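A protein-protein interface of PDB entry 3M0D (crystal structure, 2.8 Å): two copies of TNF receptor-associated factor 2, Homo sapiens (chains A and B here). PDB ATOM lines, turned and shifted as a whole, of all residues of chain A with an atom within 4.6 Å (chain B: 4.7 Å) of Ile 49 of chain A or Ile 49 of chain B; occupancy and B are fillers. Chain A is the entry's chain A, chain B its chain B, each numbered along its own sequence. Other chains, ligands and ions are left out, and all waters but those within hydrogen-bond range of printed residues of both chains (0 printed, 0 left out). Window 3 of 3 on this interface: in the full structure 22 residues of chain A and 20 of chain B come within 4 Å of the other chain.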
ATOM      1  N   ASP A  45      10.929 -26.076  -1.028  1.00  0.00           N
ATOM      2  CA  ASP A  45      10.270 -25.773  -2.289  1.00  0.00           C
ATOM      3  C   ASP A  45      11.075 -24.746  -3.075  1.00  0.00           C
ATOM      4  O   ASP A  45      11.066 -24.745  -4.296  1.00  0.00           O
ATOM      5  CB  ASP A  45       8.850 -25.271  -2.024  1.00  0.00           C
ATOM      6  CG  ASP A  45       7.982 -26.313  -1.327  1.00  0.00           C
ATOM      7  OD1 ASP A  45       8.267 -27.527  -1.486  1.00  0.00           O
ATOM      8  OD2 ASP A  45       7.015 -25.920  -0.628  1.00  0.00           O
ATOM      9  N   GLN A  46      11.778 -23.877  -2.355  1.00  0.00           N
ATOM     10  CA  GLN A  46      12.642 -22.874  -2.960  1.00  0.00           C
ATOM     11  C   GLN A  46      13.747 -23.530  -3.758  1.00  0.00           C
ATOM     12  O   GLN A  46      14.236 -22.965  -4.732  1.00  0.00           O
ATOM     13  CB  GLN A  46      13.284 -22.015  -1.877  1.00  0.00           C
ATOM     14  CG  GLN A  46      14.249 -20.964  -2.402  1.00  0.00           C
ATOM     15  CD  GLN A  46      13.619 -19.581  -2.491  1.00  0.00           C
ATOM     16  OE1 GLN A  46      12.572 -19.392  -3.119  1.00  0.00           O
ATOM     17  NE2 GLN A  46      14.256 -18.605  -1.853  1.00  0.00           N
ATOM     18  N   ASP A  47      14.153 -24.717  -3.312  1.00  0.00           N
ATOM     19  CA  ASP A  47      15.204 -25.498  -3.961  1.00  0.00           C
ATOM     20  C   ASP A  47      14.649 -26.285  -5.175  1.00  0.00           C
ATOM     21  O   ASP A  47      15.379 -26.583  -6.132  1.00  0.00           O
ATOM     22  CB  ASP A  47      15.892 -26.415  -2.928  1.00  0.00           C
ATOM     23  N   LYS A  48      13.354 -26.606  -5.111  1.00  0.00           N
ATOM     24  CA  LYS A  48      12.618 -27.248  -6.197  1.00  0.00           C
ATOM     25  C   LYS A  48      12.313 -26.251  -7.308  1.00  0.00           C
ATOM     26  O   LYS A  48      12.457 -26.568  -8.495  1.00  0.00           O
ATOM     27  CB  LYS A  48      11.304 -27.827  -5.680  1.00  0.00           C
ATOM     28  CG  LYS A  48      11.320 -29.320  -5.467  1.00  0.00           C
ATOM     29  CD  LYS A  48       9.952 -29.851  -5.037  1.00  0.00           C
ATOM     30  CE  LYS A  48       9.893 -31.363  -5.230  1.00  0.00           C
ATOM     31  NZ  LYS A  48      11.202 -32.039  -4.930  1.00  0.00           N
ATOM     32  N   ILE A  49      11.865 -25.062  -6.916  1.00  0.00           N
ATOM     33  CA  ILE A  49      11.721 -23.945  -7.839  1.00  0.00           C
ATOM     34  C   ILE A  49      13.023 -23.622  -8.572  1.00  0.00           C
ATOM     35  O   ILE A  49      13.041 -23.455  -9.788  1.00  0.00           O
ATOM     36  CB  ILE A  49      11.329 -22.673  -7.114  1.00  0.00           C
ATOM     37  CG1 ILE A  49       9.879 -22.744  -6.668  1.00  0.00           C
ATOM     38  CG2 ILE A  49      11.559 -21.469  -8.006  1.00  0.00           C
ATOM     39  CD1 ILE A  49       9.600 -21.894  -5.434  1.00  0.00           C
ATOM     40  N   GLU A  50      14.111 -23.500  -7.829  1.00  0.00           N
ATOM     41  CA  GLU A  50      15.370 -23.148  -8.455  1.00  0.00           C
ATOM     42  C   GLU A  50      15.716 -24.209  -9.484  1.00  0.00           C
ATOM     43  O   GLU A  50      16.277 -23.909 -10.532  1.00  0.00           O
ATOM     44  CB  GLU A  50      16.483 -23.005  -7.415  1.00  0.00           C
ATOM     45  CG  GLU A  50      16.465 -21.662  -6.696  1.00  0.00           C
ATOM     46  CD  GLU A  50      17.424 -21.594  -5.508  1.00  0.00           C
ATOM     47  OE1 GLU A  50      18.600 -22.010  -5.670  1.00  0.00           O
ATOM     48  OE2 GLU A  50      16.989 -21.122  -4.420  1.00  0.00           O
ATOM     49  N   ALA A  51      15.371 -25.452  -9.173  1.00  0.00           N
ATOM     50  CA  ALA A  51      15.669 -26.576 -10.040  1.00  0.00           C
ATOM     51  C   ALA A  51      14.805 -26.519 -11.295  1.00  0.00           C
ATOM     52  O   ALA A  51      15.282 -26.787 -12.402  1.00  0.00           O
ATOM     53  CB  ALA A  51      15.455 -27.874  -9.299  1.00  0.00           C
ATOM     54  N   LEU A  52      13.536 -26.170 -11.120  1.00  0.00           N
ATOM     55  CA  LEU A  52      12.669 -25.916 -12.262  1.00  0.00           C
ATOM     56  C   LEU A  52      13.151 -24.739 -13.115  1.00  0.00           C
ATOM     57  O   LEU A  52      13.324 -24.880 -14.325  1.00  0.00           O
ATOM     58  CB  LEU A  52      11.235 -25.682 -11.804  1.00  0.00           C
ATOM     59  CG  LEU A  52      10.476 -26.996 -11.731  1.00  0.00           C
ATOM     60  CD1 LEU A  52       9.017 -26.808 -11.342  1.00  0.00           C
ATOM     61  CD2 LEU A  52      10.606 -27.682 -13.068  1.00  0.00           C
ATOM     62  N   SER A  53      13.374 -23.586 -12.491  1.00  0.00           N
ATOM     63  CA  SER A  53      13.789 -22.407 -13.243  1.00  0.00           C
ATOM     64  C   SER A  53      15.076 -22.693 -14.008  1.00  0.00           C
ATOM     65  O   SER A  53      15.328 -22.123 -15.071  1.00  0.00           O
ATOM     66  CB  SER A  53      13.988 -21.206 -12.323  1.00  0.00           C
ATOM     67  OG  SER A  53      15.316 -21.168 -11.816  1.00  0.00           O
ATOM     68  N   ASP B  45       7.139 -16.742  -3.485  1.00  0.00           N
ATOM     69  CA  ASP B  45       7.257 -18.065  -4.084  1.00  0.00           C
ATOM     70  C   ASP B  45       6.161 -18.269  -5.107  1.00  0.00           C
ATOM     71  O   ASP B  45       6.403 -18.709  -6.226  1.00  0.00           O
ATOM     72  CB  ASP B  45       7.124 -19.144  -3.017  1.00  0.00           C
ATOM     73  CG  ASP B  45       8.334 -19.226  -2.113  1.00  0.00           C
ATOM     74  OD1 ASP B  45       9.438 -18.850  -2.565  1.00  0.00           O
ATOM     75  OD2 ASP B  45       8.178 -19.678  -0.954  1.00  0.00           O
ATOM     76  N   GLN B  46       4.944 -17.943  -4.701  1.00  0.00           N
ATOM     77  CA  GLN B  46       3.776 -18.104  -5.541  1.00  0.00           C
ATOM     78  C   GLN B  46       3.976 -17.350  -6.836  1.00  0.00           C
ATOM     79  O   GLN B  46       3.611 -17.808  -7.913  1.00  0.00           O
ATOM     80  CB  GLN B  46       2.578 -17.545  -4.800  1.00  0.00           C
ATOM     81  CG  GLN B  46       1.247 -17.966  -5.341  1.00  0.00           C
ATOM     82  CD  GLN B  46       0.149 -17.484  -4.447  1.00  0.00           C
ATOM     83  OE1 GLN B  46      -0.578 -16.546  -4.782  1.00  0.00           O
ATOM     84  NE2 GLN B  46       0.039 -18.098  -3.278  1.00  0.00           N
ATOM     85  N   ASP B  47       4.572 -16.177  -6.709  1.00  0.00           N
ATOM     86  CA  ASP B  47       4.859 -15.341  -7.852  1.00  0.00           C
ATOM     87  C   ASP B  47       5.901 -15.995  -8.752  1.00  0.00           C
ATOM     88  O   ASP B  47       5.804 -15.936  -9.968  1.00  0.00           O
ATOM     89  CB  ASP B  47       5.298 -13.956  -7.378  1.00  0.00           C
ATOM     90  CG  ASP B  47       4.201 -13.245  -6.598  1.00  0.00           C
ATOM     91  OD1 ASP B  47       3.047 -13.733  -6.626  1.00  0.00           O
ATOM     92  OD2 ASP B  47       4.474 -12.202  -5.966  1.00  0.00           O
ATOM     93  N   LYS B  48       6.890 -16.626  -8.139  1.00  0.00           N
ATOM     94  CA  LYS B  48       7.848 -17.450  -8.858  1.00  0.00           C
ATOM     95  C   LYS B  48       7.201 -18.656  -9.546  1.00  0.00           C
ATOM     96  O   LYS B  48       7.654 -19.068 -10.624  1.00  0.00           O
ATOM     97  CB  LYS B  48       8.954 -17.937  -7.917  1.00  0.00           C
ATOM     98  CG  LYS B  48      10.016 -16.902  -7.645  1.00  0.00           C
ATOM     99  CD  LYS B  48      11.141 -17.437  -6.786  1.00  0.00           C
ATOM    100  CE  LYS B  48      12.232 -16.374  -6.671  1.00  0.00           C
ATOM    101  NZ  LYS B  48      13.264 -16.697  -5.645  1.00  0.00           N
ATOM    102  N   ILE B  49       6.172 -19.235  -8.926  1.00  0.00           N
ATOM    103  CA  ILE B  49       5.481 -20.374  -9.522  1.00  0.00           C
ATOM    104  C   ILE B  49       4.646 -19.924 -10.715  1.00  0.00           C
ATOM    105  O   ILE B  49       4.662 -20.556 -11.777  1.00  0.00           O
ATOM    106  CB  ILE B  49       4.537 -21.065  -8.542  1.00  0.00           C
ATOM    107  CG1 ILE B  49       5.185 -21.202  -7.164  1.00  0.00           C
ATOM    108  CG2 ILE B  49       4.123 -22.427  -9.089  1.00  0.00           C
ATOM    109  CD1 ILE B  49       6.496 -21.929  -7.178  1.00  0.00           C
ATOM    110  N   GLU B  50       3.917 -18.826 -10.536  1.00  0.00           N
ATOM    111  CA  GLU B  50       3.143 -18.222 -11.623  1.00  0.00           C
ATOM    112  C   GLU B  50       4.038 -17.984 -12.866  1.00  0.00           C
ATOM    113  O   GLU B  50       3.642 -18.223 -14.000  1.00  0.00           O
ATOM    114  CB  GLU B  50       2.522 -16.912 -11.125  1.00  0.00           C
ATOM    115  CG  GLU B  50       1.431 -16.337 -11.989  1.00  0.00           C
ATOM    116  CD  GLU B  50       0.806 -15.092 -11.380  1.00  0.00           C
ATOM    117  OE1 GLU B  50       1.005 -14.870 -10.157  1.00  0.00           O
ATOM    118  OE2 GLU B  50       0.123 -14.336 -12.122  1.00  0.00           O
ATOM    119  N   ALA B  51       5.260 -17.528 -12.625  1.00  0.00           N
ATOM    120  CA  ALA B  51       6.210 -17.206 -13.671  1.00  0.00           C
ATOM    121  C   ALA B  51       6.706 -18.460 -14.376  1.00  0.00           C
ATOM    122  O   ALA B  51       6.761 -18.517 -15.598  1.00  0.00           O
ATOM    123  CB  ALA B  51       7.383 -16.443 -13.065  1.00  0.00           C
ATOM    124  N   LEU B  52       7.093 -19.450 -13.585  1.00  0.00           N
ATOM    125  CA  LEU B  52       7.541 -20.731 -14.106  1.00  0.00           C
ATOM    126  C   LEU B  52       6.387 -21.394 -14.842  1.00  0.00           C
ATOM    127  O   LEU B  52       6.575 -22.155 -15.780  1.00  0.00           O
ATOM    128  CB  LEU B  52       8.003 -21.628 -12.948  1.00  0.00           C
ATOM    129  CG  LEU B  52       9.468 -22.031 -12.786  1.00  0.00           C
ATOM    130  CD1 LEU B  52      10.399 -20.910 -13.153  1.00  0.00           C
ATOM    131  CD2 LEU B  52       9.707 -22.446 -11.364  1.00  0.00           C
ATOM    132  N   SER B  53       5.176 -21.110 -14.392  1.00  0.00           N
ATOM    133  CA  SER B  53       4.006 -21.740 -14.969  1.00  0.00           C
ATOM    134  C   SER B  53       3.759 -21.126 -16.342  1.00  0.00           C
ATOM    135  O   SER B  53       3.469 -21.823 -17.315  1.00  0.00           O
ATOM    136  CB  SER B  53       2.806 -21.515 -14.058  1.00  0.00           C
ATOM    137  OG  SER B  53       1.776 -22.415 -14.381  1.00  0.00           O
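The side-chain carboxylate of Asp 45 of chain B lies close to the side-chain amide oxygen of Gln 46 of chain A (3.2 Å).
Ile 49 of chain A touches two residues of chain B. Of the printed residues of chain B, Leu 52 of chain A touches Leu 52 (3.6 Å). Of the printed residues of chain A, Asp 45 of chain B touches Gln 46. Of the printed residues of chain A, Lys 48 of chain B touches Gln 46 (3.8 Å). Ile 49 of chain B touches just one residue of chain A: Ile 49 (3.5 Å). The nearest residue of chain B that does not touch Ile 49 of chain A is Asp 45 of chain B (4.2 Å). The nearest printed residue of chain A that does not touch Leu 52 of chain B is Lys 48 of chain A (5.7 Å).
Of the 9 printed residues of chain B, 4 touch a printed residue of chain A. Printed residues of chain B that touch a printed residue of chain A: Asp 45, Lys 48, Ile 49 and Leu 52. Hydrophobic or aromatic side chains of chain B that line the printed part of chain A: Ile 49 and Leu 52. Printed residues of chain A that touch a printed residue of chain B: Gln 46, Ile 49, Leu 52 and Ser 53. Hydrophobic or aromatic side chains of chain A that line the printed part of chain B: Ile 49 and Leu 52. Among the printed residues, no Asp or Glu carboxylate lies within 4 Å of a Lys or Arg side-chain nitrogen of the other chain.
Gln 46 of chain A touches Lys 48 of chain B, but with the chains exchanged Lys 48 of chain A does not touch Gln 46 of chain B (11.4 Å). Ile 49 of chain A touches its own counterpart, Ile 49 of chain B. Ile 49 of chain A touches Leu 52 of chain B, but with the chains exchanged Leu 52 of chain A does not touch Ile 49 of chain B (6.9 Å). Leu 52 of chain A touches its own counterpart, Leu 52 of chain B. 9 positions are printed for both chains. Of the 6 pairs that touch across the chains among the printed residues, 2 have their exchanged pair printed and touching as well.
The backbone carbonyl oxygen of Glu 50 of chain A sits at hydrogen-bond distance from the side-chain hydroxyl of Ser 53 of chain A.
Gln 46 of chain A touches Lys 48 of chain B. Ile 49 of chain B touches Ile 49 of chain A. Ile 49 of chain A touches Leu 52 of chain B. CB of Leu 52 of chain A touches CD2 of Leu 52 of chain B, at 3.6 Å. Leu 52 of chain B touches Ser 53 of chain A.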
